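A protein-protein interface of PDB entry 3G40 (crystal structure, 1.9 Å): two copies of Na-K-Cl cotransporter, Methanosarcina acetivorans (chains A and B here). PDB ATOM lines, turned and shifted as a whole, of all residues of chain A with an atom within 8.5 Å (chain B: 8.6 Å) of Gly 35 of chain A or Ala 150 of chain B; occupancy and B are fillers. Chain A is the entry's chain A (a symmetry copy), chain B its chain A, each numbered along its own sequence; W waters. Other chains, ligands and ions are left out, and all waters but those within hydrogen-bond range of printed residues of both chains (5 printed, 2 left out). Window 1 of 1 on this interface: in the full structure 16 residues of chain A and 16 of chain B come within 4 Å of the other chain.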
ATOM      1  N   ASP A  29      30.440 -18.057 -11.363  1.00  0.00           N
ATOM      2  CA  ASP A  29      30.701 -19.491 -11.324  1.00  0.00           C
ATOM      3  C   ASP A  29      30.923 -19.977 -12.749  1.00  0.00           C
ATOM      4  O   ASP A  29      29.994 -19.947 -13.557  1.00  0.00           O
ATOM      5  CB  ASP A  29      29.492 -20.213 -10.698  1.00  0.00           C
ATOM      6  CG  ASP A  29      29.612 -21.738 -10.749  1.00  0.00           C
ATOM      7  OD1 ASP A  29      30.690 -22.244 -11.114  1.00  0.00           O
ATOM      8  OD2 ASP A  29      28.621 -22.433 -10.424  1.00  0.00           O
ATOM      9  N   PRO A  30      32.149 -20.431 -13.059  1.00  0.00           N
ATOM     10  CA  PRO A  30      32.517 -20.813 -14.425  1.00  0.00           C
ATOM     11  C   PRO A  30      31.737 -22.030 -14.921  1.00  0.00           C
ATOM     12  O   PRO A  30      31.627 -22.218 -16.132  1.00  0.00           O
ATOM     13  CB  PRO A  30      34.005 -21.169 -14.306  1.00  0.00           C
ATOM     14  CG  PRO A  30      34.445 -20.573 -13.029  1.00  0.00           C
ATOM     15  CD  PRO A  30      33.276 -20.595 -12.124  1.00  0.00           C
ATOM     16  N   ARG A  31      31.233 -22.851 -14.003  1.00  0.00           N
ATOM     17  CA  ARG A  31      30.435 -24.017 -14.378  1.00  0.00           C
ATOM     18  C   ARG A  31      29.094 -23.604 -14.985  1.00  0.00           C
ATOM     19  O   ARG A  31      28.621 -24.227 -15.938  1.00  0.00           O
ATOM     20  CB  ARG A  31      30.202 -24.922 -13.169  1.00  0.00           C
ATOM     21  CG  ARG A  31      31.486 -25.497 -12.568  1.00  0.00           C
ATOM     22  CD  ARG A  31      31.213 -25.945 -11.145  1.00  0.00           C
ATOM     23  NE  ARG A  31      32.430 -26.328 -10.441  1.00  0.00           N
ATOM     24  CZ  ARG A  31      32.540 -26.352  -9.118  1.00  0.00           C
ATOM     25  NH1 ARG A  31      31.505 -26.005  -8.363  1.00  0.00           N
ATOM     26  NH2 ARG A  31      33.682 -26.715  -8.552  1.00  0.00           N
ATOM     27  N   GLU A  32      28.479 -22.564 -14.425  1.00  0.00           N
ATOM     28  CA  GLU A  32      27.262 -21.994 -15.005  1.00  0.00           C
ATOM     29  C   GLU A  32      27.560 -21.447 -16.386  1.00  0.00           C
ATOM     30  O   GLU A  32      26.786 -21.635 -17.324  1.00  0.00           O
ATOM     31  CB  GLU A  32      26.701 -20.871 -14.131  1.00  0.00           C
ATOM     32  CG  GLU A  32      25.888 -21.339 -12.941  1.00  0.00           C
ATOM     33  CD  GLU A  32      24.476 -21.793 -13.308  1.00  0.00           C
ATOM     34  OE1 GLU A  32      24.056 -21.645 -14.482  1.00  0.00           O
ATOM     35  OE2 GLU A  32      23.779 -22.296 -12.403  1.00  0.00           O
ATOM     36  N   LEU A  33      28.686 -20.755 -16.515  1.00  0.00           N
ATOM     37  CA  LEU A  33      29.099 -20.264 -17.823  1.00  0.00           C
ATOM     38  C   LEU A  33      29.245 -21.413 -18.818  1.00  0.00           C
ATOM     39  O   LEU A  33      28.770 -21.309 -19.941  1.00  0.00           O
ATOM     40  CB  LEU A  33      30.413 -19.481 -17.723  1.00  0.00           C
ATOM     41  CG  LEU A  33      30.996 -18.989 -19.049  1.00  0.00           C
ATOM     42  CD1 LEU A  33      30.006 -18.099 -19.788  1.00  0.00           C
ATOM     43  CD2 LEU A  33      32.335 -18.243 -18.792  1.00  0.00           C
ATOM     44  N   MET A  34      29.920 -22.494 -18.422  1.00  0.00           N
ATOM     45  CA  MET A  34      30.092 -23.639 -19.311  1.00  0.00           C
ATOM     46  C   MET A  34      28.708 -24.187 -19.719  1.00  0.00           C
ATOM     47  O   MET A  34      28.508 -24.615 -20.857  1.00  0.00           O
ATOM     48  CB  MET A  34      30.914 -24.742 -18.650  1.00  0.00           C
ATOM     49  CG  MET A  34      32.418 -24.400 -18.515  1.00  0.00           C
ATOM     50  SD  MET A  34      33.146 -23.960 -20.119  1.00  0.00           S
ATOM     51  CE  MET A  34      33.217 -25.550 -20.921  1.00  0.00           C
ATOM     52  N   GLY A  35      27.766 -24.169 -18.786  1.00  0.00           N
ATOM     53  CA  GLY A  35      26.429 -24.683 -19.065  1.00  0.00           C
ATOM     54  C   GLY A  35      25.625 -23.795 -20.006  1.00  0.00           C
ATOM     55  O   GLY A  35      24.612 -24.225 -20.560  1.00  0.00           O
ATOM     56  N   THR A  36      26.087 -22.559 -20.191  1.00  0.00           N
ATOM     57  CA  THR A  36      25.386 -21.565 -20.997  1.00  0.00           C
ATOM     58  C   THR A  36      26.175 -21.204 -22.245  1.00  0.00           C
ATOM     59  O   THR A  36      25.689 -20.456 -23.080  1.00  0.00           O
ATOM     60  CB  THR A  36      25.167 -20.248 -20.211  1.00  0.00           C
ATOM     61  OG1 THR A  36      24.811 -20.538 -18.857  1.00  0.00           O
ATOM     62  CG2 THR A  36      24.071 -19.420 -20.854  1.00  0.00           C
ATOM     63  N   PHE A  37      27.403 -21.720 -22.368  1.00  0.00           N
ATOM     64  CA  PHE A  37      28.271 -21.361 -23.489  1.00  0.00           C
ATOM     65  C   PHE A  37      27.571 -21.463 -24.856  1.00  0.00           C
ATOM     66  O   PHE A  37      27.601 -20.524 -25.656  1.00  0.00           O
ATOM     67  CB  PHE A  37      29.537 -22.234 -23.473  1.00  0.00           C
ATOM     68  CG  PHE A  37      30.524 -21.914 -24.559  1.00  0.00           C
ATOM     69  CD1 PHE A  37      31.676 -21.168 -24.252  1.00  0.00           C
ATOM     70  CD2 PHE A  37      30.373 -22.419 -25.847  1.00  0.00           C
ATOM     71  CE1 PHE A  37      32.635 -20.895 -25.234  1.00  0.00           C
ATOM     72  CE2 PHE A  37      31.311 -22.139 -26.837  1.00  0.00           C
ATOM     73  CZ  PHE A  37      32.462 -21.375 -26.520  1.00  0.00           C
ATOM     74  N   ASP A  38      26.962 -22.605 -25.143  1.00  0.00           N
ATOM     75  CA  ASP A  38      26.417 -22.813 -26.488  1.00  0.00           C
ATOM     76  C   ASP A  38      25.285 -21.842 -26.799  1.00  0.00           C
ATOM     77  O   ASP A  38      25.109 -21.405 -27.935  1.00  0.00           O
ATOM     78  CB  ASP A  38      25.960 -24.266 -26.686  1.00  0.00           C
ATOM     79  CG  ASP A  38      27.118 -25.216 -26.929  1.00  0.00           C
ATOM     80  OD1 ASP A  38      28.240 -24.747 -27.246  1.00  0.00           O
ATOM     81  OD2 ASP A  38      26.912 -26.441 -26.815  1.00  0.00           O
ATOM     82  N   PHE A  39      24.510 -21.531 -25.776  1.00  0.00           N
ATOM     83  CA  PHE A  39      23.377 -20.625 -25.910  1.00  0.00           C
ATOM     84  C   PHE A  39      23.892 -19.202 -26.134  1.00  0.00           C
ATOM     85  O   PHE A  39      23.390 -18.483 -26.992  1.00  0.00           O
ATOM     86  CB  PHE A  39      22.493 -20.714 -24.660  1.00  0.00           C
ATOM     87  CG  PHE A  39      21.216 -19.897 -24.740  1.00  0.00           C
ATOM     88  CD1 PHE A  39      20.324 -20.069 -25.793  1.00  0.00           C
ATOM     89  CD2 PHE A  39      20.909 -18.979 -23.753  1.00  0.00           C
ATOM     90  CE1 PHE A  39      19.153 -19.322 -25.865  1.00  0.00           C
ATOM     91  CE2 PHE A  39      19.744 -18.229 -23.803  1.00  0.00           C
ATOM     92  CZ  PHE A  39      18.852 -18.406 -24.871  1.00  0.00           C
ATOM     93  N   LEU A  40      24.906 -18.790 -25.370  1.00  0.00           N
ATOM     94  CA  LEU A  40      25.506 -17.475 -25.590  1.00  0.00           C
ATOM     95  C   LEU A  40      26.061 -17.431 -27.008  1.00  0.00           C
ATOM     96  O   LEU A  40      25.934 -16.425 -27.702  1.00  0.00           O
ATOM     97  CB  LEU A  40      26.641 -17.210 -24.566  1.00  0.00           C
ATOM     98  CG  LEU A  40      26.158 -17.037 -23.127  1.00  0.00           C
ATOM     99  CD1 LEU A  40      27.310 -17.083 -22.095  1.00  0.00           C
ATOM    100  CD2 LEU A  40      25.366 -15.752 -22.985  1.00  0.00           C
ATOM    101  N   ILE A  71      37.769 -19.962 -21.660  1.00  0.00           N
ATOM    102  CA  ILE A  71      36.416 -19.930 -22.197  1.00  0.00           C
ATOM    103  C   ILE A  71      36.314 -18.827 -23.241  1.00  0.00           C
ATOM    104  O   ILE A  71      35.699 -19.003 -24.282  1.00  0.00           O
ATOM    105  CB  ILE A  71      35.373 -19.793 -21.089  1.00  0.00           C
ATOM    106  CG1 ILE A  71      35.532 -20.964 -20.113  1.00  0.00           C
ATOM    107  CG2 ILE A  71      33.948 -19.800 -21.685  1.00  0.00           C
ATOM    108  CD1 ILE A  71      34.773 -20.802 -18.825  1.00  0.00           C
ATOM    109  N   PHE A 144      17.658 -14.606 -18.526  1.00  0.00           N
ATOM    110  CA  PHE A 144      17.469 -15.986 -18.942  1.00  0.00           C
ATOM    111  C   PHE A 144      16.991 -16.881 -17.799  1.00  0.00           C
ATOM    112  O   PHE A 144      17.622 -16.965 -16.748  1.00  0.00           O
ATOM    113  CB  PHE A 144      18.773 -16.495 -19.558  1.00  0.00           C
ATOM    114  CG  PHE A 144      18.729 -17.922 -20.027  1.00  0.00           C
ATOM    115  CD1 PHE A 144      17.622 -18.424 -20.720  1.00  0.00           C
ATOM    116  CD2 PHE A 144      19.818 -18.751 -19.815  1.00  0.00           C
ATOM    117  CE1 PHE A 144      17.608 -19.738 -21.165  1.00  0.00           C
ATOM    118  CE2 PHE A 144      19.816 -20.060 -20.262  1.00  0.00           C
ATOM    119  CZ  PHE A 144      18.708 -20.560 -20.935  1.00  0.00           C
ATOM    120  N   LYS A 146      16.406 -20.556 -17.289  1.00  0.00           N
ATOM    121  CA  LYS A 146      16.581 -21.881 -17.870  1.00  0.00           C
ATOM    122  C   LYS A 146      15.834 -22.916 -17.057  1.00  0.00           C
ATOM    123  O   LYS A 146      16.004 -22.998 -15.846  1.00  0.00           O
ATOM    124  CB  LYS A 146      18.071 -22.250 -17.956  1.00  0.00           C
ATOM    125  CG  LYS A 146      18.294 -23.633 -18.544  1.00  0.00           C
ATOM    126  CD  LYS A 146      19.684 -23.778 -19.180  1.00  0.00           C
ATOM    127  CE  LYS A 146      20.669 -24.414 -18.235  1.00  0.00           C
ATOM    128  NZ  LYS A 146      21.930 -24.778 -18.957  1.00  0.00           N
ATOM    129  N   GLY A 151      15.868 -27.729 -19.682  1.00  0.00           N
ATOM    130  CA  GLY A 151      16.892 -26.911 -20.315  1.00  0.00           C
ATOM    131  C   GLY A 151      16.306 -26.305 -21.584  1.00  0.00           C
ATOM    132  O   GLY A 151      15.174 -25.815 -21.566  1.00  0.00           O
ATOM    133  N   LEU A 152      17.051 -26.346 -22.689  1.00  0.00           N
ATOM    134  CA  LEU A 152      16.543 -25.802 -23.948  1.00  0.00           C
ATOM    135  C   LEU A 152      15.934 -26.908 -24.792  1.00  0.00           C
ATOM    136  O   LEU A 152      15.593 -26.697 -25.957  1.00  0.00           O
ATOM    137  CB  LEU A 152      17.652 -25.075 -24.719  1.00  0.00           C
ATOM    138  CG  LEU A 152      18.180 -23.829 -24.005  1.00  0.00           C
ATOM    139  CD1 LEU A 152      19.470 -23.321 -24.623  1.00  0.00           C
ATOM    140  CD2 LEU A 152      17.111 -22.738 -24.002  1.00  0.00           C
ATOM    141  N   GLN A 155      15.542 -27.571 -28.793  1.00  0.00           N
ATOM    142  CA  GLN A 155      15.856 -26.332 -29.528  1.00  0.00           C
ATOM    143  C   GLN A 155      15.217 -26.328 -30.919  1.00  0.00           C
ATOM    144  O   GLN A 155      15.855 -25.958 -31.904  1.00  0.00           O
ATOM    145  CB  GLN A 155      17.383 -26.136 -29.640  1.00  0.00           C
ATOM    146  CG  GLN A 155      18.057 -26.216 -28.300  1.00  0.00           C
ATOM    147  CD  GLN A 155      19.563 -25.850 -28.302  1.00  0.00           C
ATOM    148  OE1 GLN A 155      20.158 -25.551 -29.334  1.00  0.00           O
ATOM    149  NE2 GLN A 155      20.165 -25.897 -27.133  1.00  0.00           N
ATOM    150  N   LYS B 146      24.156 -35.736 -14.513  1.00  0.00           N
ATOM    151  CA  LYS B 146      24.311 -34.481 -15.237  1.00  0.00           C
ATOM    152  C   LYS B 146      24.609 -33.350 -14.276  1.00  0.00           C
ATOM    153  O   LYS B 146      23.888 -33.152 -13.305  1.00  0.00           O
ATOM    154  CB  LYS B 146      23.050 -34.160 -16.056  1.00  0.00           C
ATOM    155  CG  LYS B 146      23.168 -32.849 -16.816  1.00  0.00           C
ATOM    156  CD  LYS B 146      22.251 -32.805 -18.046  1.00  0.00           C
ATOM    157  CE  LYS B 146      20.952 -32.103 -17.751  1.00  0.00           C
ATOM    158  NZ  LYS B 146      20.194 -31.845 -19.017  1.00  0.00           N
ATOM    159  N   HIS B 147      25.682 -32.610 -14.528  1.00  0.00           N
ATOM    160  CA  HIS B 147      26.039 -31.525 -13.624  1.00  0.00           C
ATOM    161  C   HIS B 147      24.994 -30.421 -13.690  1.00  0.00           C
ATOM    162  O   HIS B 147      24.640 -29.968 -14.780  1.00  0.00           O
ATOM    163  CB  HIS B 147      27.426 -30.965 -13.952  1.00  0.00           C
ATOM    164  CG  HIS B 147      27.978 -30.097 -12.870  1.00  0.00           C
ATOM    165  ND1 HIS B 147      27.603 -28.780 -12.716  1.00  0.00           N
ATOM    166  CD2 HIS B 147      28.832 -30.367 -11.856  1.00  0.00           C
ATOM    167  CE1 HIS B 147      28.223 -28.269 -11.667  1.00  0.00           C
ATOM    168  NE2 HIS B 147      28.973 -29.214 -11.126  1.00  0.00           N
ATOM    169  N   PRO B 148      24.497 -29.979 -12.520  1.00  0.00           N
ATOM    170  CA  PRO B 148      23.352 -29.056 -12.432  1.00  0.00           C
ATOM    171  C   PRO B 148      23.658 -27.665 -12.966  1.00  0.00           C
ATOM    172  O   PRO B 148      22.727 -26.931 -13.267  1.00  0.00           O
ATOM    173  CB  PRO B 148      23.063 -28.974 -10.929  1.00  0.00           C
ATOM    174  CG  PRO B 148      23.862 -30.058 -10.296  1.00  0.00           C
ATOM    175  CD  PRO B 148      25.003 -30.371 -11.199  1.00  0.00           C
ATOM    176  N   GLN B 149      24.933 -27.310 -13.081  1.00  0.00           N
ATOM    177  CA  GLN B 149      25.305 -26.013 -13.653  1.00  0.00           C
ATOM    178  C   GLN B 149      25.916 -26.162 -15.044  1.00  0.00           C
ATOM    179  O   GLN B 149      25.525 -25.466 -15.978  1.00  0.00           O
ATOM    180  CB  GLN B 149      26.299 -25.275 -12.750  1.00  0.00           C
ATOM    181  CG  GLN B 149      25.668 -24.601 -11.539  1.00  0.00           C
ATOM    182  CD  GLN B 149      25.440 -25.556 -10.386  1.00  0.00           C
ATOM    183  OE1 GLN B 149      26.351 -26.266  -9.961  1.00  0.00           O
ATOM    184  NE2 GLN B 149      24.218 -25.568  -9.863  1.00  0.00           N
ATOM    185  N   ALA B 150      26.901 -27.046 -15.163  1.00  0.00           N
ATOM    186  CA  ALA B 150      27.648 -27.191 -16.411  1.00  0.00           C
ATOM    187  C   ALA B 150      26.898 -27.990 -17.477  1.00  0.00           C
ATOM    188  O   ALA B 150      27.196 -27.857 -18.659  1.00  0.00           O
ATOM    189  CB  ALA B 150      29.010 -27.830 -16.153  1.00  0.00           C
ATOM    190  N   GLY B 151      25.948 -28.829 -17.072  1.00  0.00           N
ATOM    191  CA  GLY B 151      25.326 -29.732 -18.030  1.00  0.00           C
ATOM    192  C   GLY B 151      26.428 -30.448 -18.799  1.00  0.00           C
ATOM    193  O   GLY B 151      27.403 -30.904 -18.198  1.00  0.00           O
ATOM    194  N   LEU B 152      26.297 -30.538 -20.123  1.00  0.00           N
ATOM    195  CA  LEU B 152      27.327 -31.192 -20.929  1.00  0.00           C
ATOM    196  C   LEU B 152      28.292 -30.162 -21.489  1.00  0.00           C
ATOM    197  O   LEU B 152      29.140 -30.481 -22.326  1.00  0.00           O
ATOM    198  CB  LEU B 152      26.699 -32.021 -22.057  1.00  0.00           C
ATOM    199  CG  LEU B 152      25.864 -33.203 -21.556  1.00  0.00           C
ATOM    200  CD1 LEU B 152      25.009 -33.804 -22.658  1.00  0.00           C
ATOM    201  CD2 LEU B 152      26.776 -34.260 -20.937  1.00  0.00           C
ATOM    202  N   GLY B 153      28.161 -28.922 -21.028  1.00  0.00           N
ATOM    203  CA  GLY B 153      29.147 -27.892 -21.341  1.00  0.00           C
ATOM    204  C   GLY B 153      29.291 -27.704 -22.835  1.00  0.00           C
ATOM    205  O   GLY B 153      28.293 -27.633 -23.565  1.00  0.00           O
ATOM    206  N   ARG B 154      30.530 -27.662 -23.311  1.00  0.00           N
ATOM    207  CA  ARG B 154      30.770 -27.456 -24.734  1.00  0.00           C
ATOM    208  C   ARG B 154      30.748 -28.760 -25.540  1.00  0.00           C
ATOM    209  O   ARG B 154      30.922 -28.728 -26.748  1.00  0.00           O
ATOM    210  CB  ARG B 154      32.097 -26.707 -24.960  1.00  0.00           C
ATOM    211  CG  ARG B 154      32.094 -25.259 -24.457  1.00  0.00           C
ATOM    212  CD  ARG B 154      33.498 -24.614 -24.584  1.00  0.00           C
ATOM    213  NE  ARG B 154      33.941 -24.507 -25.974  1.00  0.00           N
ATOM    214  CZ  ARG B 154      35.214 -24.369 -26.344  1.00  0.00           C
ATOM    215  NH1 ARG B 154      36.182 -24.328 -25.436  1.00  0.00           N
ATOM    216  NH2 ARG B 154      35.524 -24.273 -27.623  1.00  0.00           N
ATOM    217  N   GLN B 155      30.552 -29.896 -24.870  1.00  0.00           N
ATOM    218  CA  GLN B 155      30.593 -31.209 -25.537  1.00  0.00           C
ATOM    219  C   GLN B 155      31.815 -31.337 -26.450  1.00  0.00           C
ATOM    220  O   GLN B 155      31.712 -31.822 -27.576  1.00  0.00           O
ATOM    221  CB  GLN B 155      29.297 -31.454 -26.339  1.00  0.00           C
ATOM    222  CG  GLN B 155      28.070 -31.258 -25.495  1.00  0.00           C
ATOM    223  CD  GLN B 155      26.737 -31.660 -26.174  1.00  0.00           C
ATOM    224  OE1 GLN B 155      26.696 -32.077 -27.330  1.00  0.00           O
ATOM    225  NE2 GLN B 155      25.654 -31.511 -25.443  1.00  0.00           N
ATOM    226  N   PHE B 244      40.242 -31.866 -16.727  1.00  0.00           N
ATOM    227  CA  PHE B 244      38.946 -31.353 -17.179  1.00  0.00           C
ATOM    228  C   PHE B 244      38.362 -32.067 -18.408  1.00  0.00           C
ATOM    229  O   PHE B 244      39.087 -32.387 -19.351  1.00  0.00           O
ATOM    230  CB  PHE B 244      38.998 -29.854 -17.458  1.00  0.00           C
ATOM    231  CG  PHE B 244      37.674 -29.315 -17.933  1.00  0.00           C
ATOM    232  CD1 PHE B 244      36.681 -28.998 -17.022  1.00  0.00           C
ATOM    233  CD2 PHE B 244      37.401 -29.191 -19.291  1.00  0.00           C
ATOM    234  CE1 PHE B 244      35.440 -28.530 -17.451  1.00  0.00           C
ATOM    235  CE2 PHE B 244      36.163 -28.728 -19.726  1.00  0.00           C
ATOM    236  CZ  PHE B 244      35.187 -28.394 -18.802  1.00  0.00           C
ATOM    237  N   ALA B 245      37.051 -32.307 -18.392  1.00  0.00           N
ATOM    238  CA  ALA B 245      36.328 -32.795 -19.580  1.00  0.00           C
ATOM    239  C   ALA B 245      34.868 -32.316 -19.568  1.00  0.00           C
ATOM    240  O   ALA B 245      34.334 -32.017 -18.514  1.00  0.00           O
ATOM    241  CB  ALA B 245      36.359 -34.316 -19.662  1.00  0.00           C
ATOM    242  N   SER B 246      34.232 -32.257 -20.739  1.00  0.00           N
ATOM    243  CA  SER B 246      32.782 -32.004 -20.828  1.00  0.00           C
ATOM    244  C   SER B 246      32.030 -33.154 -20.193  1.00  0.00           C
ATOM    245  O   SER B 246      30.982 -32.980 -19.544  1.00  0.00           O
ATOM    246  CB  SER B 246      32.353 -31.886 -22.295  1.00  0.00           C
ATOM    247  OG  SER B 246      33.140 -30.916 -22.994  1.00  0.00           O
ATOM    248  N   LEU B 247      32.564 -34.346 -20.392  1.00  0.00           N
ATOM    249  CA  LEU B 247      31.937 -35.552 -19.881  1.00  0.00           C
ATOM    250  C   LEU B 247      33.002 -36.554 -19.491  1.00  0.00           C
ATOM    251  O   LEU B 247      33.890 -36.875 -20.294  1.00  0.00           O
ATOM    252  CB  LEU B 247      31.043 -36.188 -20.946  1.00  0.00           C
ATOM    253  CG  LEU B 247      30.381 -37.523 -20.546  1.00  0.00           C
ATOM    254  CD1 LEU B 247      29.279 -37.331 -19.495  1.00  0.00           C
ATOM    255  CD2 LEU B 247      29.809 -38.250 -21.769  1.00  0.00           C
ATOM    256  N   MET B 265      31.115 -36.426  -9.753  1.00  0.00           N
ATOM    257  CA  MET B 265      30.551 -35.389 -10.596  1.00  0.00           C
ATOM    258  C   MET B 265      30.770 -34.010  -9.980  1.00  0.00           C
ATOM    259  O   MET B 265      31.106 -33.057 -10.677  1.00  0.00           O
ATOM    260  CB  MET B 265      29.059 -35.647 -10.870  1.00  0.00           C
ATOM    261  CG  MET B 265      28.420 -34.529 -11.676  1.00  0.00           C
ATOM    262  SD  MET B 265      27.568 -33.371 -10.596  1.00  0.00           S
ATOM    263  CE  MET B 265      26.132 -34.352 -10.197  1.00  0.00           C
ATOM    264  N   ALA B 268      34.477 -33.092 -10.236  1.00  0.00           N
ATOM    265  CA  ALA B 268      34.778 -32.799 -11.635  1.00  0.00           C
ATOM    266  C   ALA B 268      34.291 -31.421 -12.073  1.00  0.00           C
ATOM    267  O   ALA B 268      34.928 -30.759 -12.898  1.00  0.00           O
ATOM    268  CB  ALA B 268      34.165 -33.869 -12.527  1.00  0.00           C
ATOM    269  N   GLY B 269      33.150 -30.996 -11.535  1.00  0.00           N
ATOM    270  CA  GLY B 269      32.545 -29.747 -11.953  1.00  0.00           C
ATOM    271  C   GLY B 269      31.941 -29.896 -13.338  1.00  0.00           C
ATOM    272  O   GLY B 269      31.670 -28.906 -14.020  1.00  0.00           O
ATOM    273  N   SER B 270      31.735 -31.144 -13.754  1.00  0.00           N
ATOM    274  CA  SER B 270      31.127 -31.432 -15.045  1.00  0.00           C
ATOM    275  C   SER B 270      30.419 -32.790 -15.014  1.00  0.00           C
ATOM    276  O   SER B 270      30.543 -33.537 -14.044  1.00  0.00           O
ATOM    277  CB  SER B 270      32.191 -31.408 -16.134  1.00  0.00           C
ATOM    278  OG  SER B 270      33.114 -32.437 -15.903  1.00  0.00           O
ATOM    279  N   SER B 271      29.713 -33.129 -16.085  1.00  0.00           N
ATOM    280  CA  SER B 271      28.889 -34.335 -16.077  1.00  0.00           C
ATOM    281  C   SER B 271      29.671 -35.649 -16.133  1.00  0.00           C
ATOM    282  O   SER B 271      30.753 -35.737 -16.699  1.00  0.00           O
ATOM    283  CB  SER B 271      27.846 -34.297 -17.196  1.00  0.00           C
ATOM    284  OG  SER B 271      26.958 -33.208 -17.023  1.00  0.00           O
HETATM  285  O   HOH W   1      30.662 -29.086  -8.852  1.00  0.00           O
HETATM  286  O   HOH W   2      22.980 -26.948 -17.636  1.00  0.00           O
HETATM  287  O   HOH W   3      23.501 -23.668 -16.438  1.00  0.00           O
HETATM  288  O   HOH W   4      21.507 -23.712 -13.187  1.00  0.00           O
HETATM  289  O   HOH W   5      26.973 -25.020 -23.202  1.00  0.00           O
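O of Arg 31 of chain A sits close to N of Ala 150 of chain B (3.4 Å).
The backbone carbonyl oxygen (O) of Arg 31 of chain A sits close to the backbone carbonyl oxygen (O) of Gln 149 of chain B, at 3.3 Å.
A ring nitrogen (ND1) of His 147 of chain B lies within hydrogen-bond range of the backbone NH (N) of Gln 149 of chain B (3.1 Å).
A ring nitrogen (ND1) of His 147 of chain B is in hydrogen-bond range of the backbone NH (N) of Ala 150 of chain B (3.1 Å).
The side-chain hydroxyl (OG) of Ser 271 of chain B is in hydrogen-bond range of the backbone NH (N) of His 147 of chain B.
The side-chain carboxylate of Asp 29 of chain A sits at hydrogen-bond distance from the backbone NH of Arg 31 of chain A (3.0 Å).
O of Glu 32 of chain A lies within hydrogen-bond range of OG1 of Thr 36 of chain A.
O of Gly 35 of chain A is in hydrogen-bond range of NZ of Lys 146 of chain A (3.2 Å).
CG of Gln 149 of chain B touches OD2 of Asp 29 of chain A (3.8 Å).
His 147 of chain B touches Arg 31 of chain A (CE1 to CD, 3.8 Å).
O of Gly 269 of chain B touches CG of Arg 31 of chain A (3.7 Å).
Glu 32 of chain A touches Gln 149 of chain B (OE2 to CG, 3.1 Å).
Gly 153 of chain B touches Met 34 of chain A.
CE of Met 34 of chain A touches CG of Arg 154 of chain B, 3.7 Å away.
CA of Gly 35 of chain A touches O of Gln 149 of chain B (3.3 Å).
Ala 150 of chain B touches Gly 35 of chain A (O to CA, 3.3 Å).
Phe 37 of chain A touches Arg 154 of chain B (CZ to NE, 3.5 Å).
Asp 38 of chain A touches Gly 153 of chain B (OD2 to O, 3.7 Å).
Of the printed residues of chain B, Met 34 of chain A touches Gly 153 and Arg 154.
Of chain B, only Gln 149 (3.3 Å) and Ala 150 (3.3 Å) come within 4 Å of Gly 35 of chain A.
Of the printed residues of chain B, Asp 38 of chain A touches Gly 153 (3.7 Å).
Phe 39 of chain A touches none of the printed residues of chain B.
Gly 151 of chain A touches none of the printed residues of chain B.
Of the printed residues of chain A, Gln 149 of chain B touches Asp 29 (3.8 Å), Arg 31 (3.3 Å), Glu 32 (3.1 Å) and Gly 35 (3.3 Å).
Ala 150 of chain B touches just these residues of chain A: Arg 31 (3.2 Å) and Gly 35 (3.3 Å).
No residue of chain A comes within 4 Å of Gly 151 of chain B.
Of the printed residues of chain A, Arg 154 of chain B touches Met 34 (3.7 Å) and Phe 37 (3.5 Å).
The nearest residue of chain B that does not touch Gly 35 of chain A is Gly 151 of chain B (4.6 Å).
Of the 19 printed residues of chain B, 6 touch a printed residue of chain A.
Along chain B the printed residues that touch a printed residue of chain A span positions 147 to 269.
Hydrophobic or aromatic side chains of chain A within 4 Å of the printed part of chain B: Met 34 and Phe 37.
Positions printed for both chains: 146, 151, 152 and 155.
Of the 12 pairs that touch across the chains among the printed residues, none has its exchanged pair printed and touching as well.
Water W3 lies within hydrogen-bond range of the backbone carbonyl oxygen of Gln 149 of chain B, the side-chain carboxylate of Glu 32 of chain A and the side-chain amino group of Lys 146 of chain A.
Water W2 lies within hydrogen-bond range of the side-chain amino group of Lys 146 of chain A (2.7 Å) and the backbone carbonyl oxygen of Gln 149 of chain B (3.4 Å).
Water W4 lies within hydrogen-bond range of OE2 of Glu 32 of chain A and O of Pro 148 of chain B.
Water W5 lies within hydrogen-bond range of the backbone carbonyl oxygen (O) of Met 34 of chain A, the backbone carbonyl oxygen (O) of Gly 153 of chain B, the backbone NH (N) of Asp 38 of chain A and the backbone NH (N) of Phe 37 of chain A.
Water W1 bridges a ring nitrogen (NE2) of His 147 of chain B (2.8 Å) and the guanidinium group of Arg 31 of chain A (3.2 Å).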
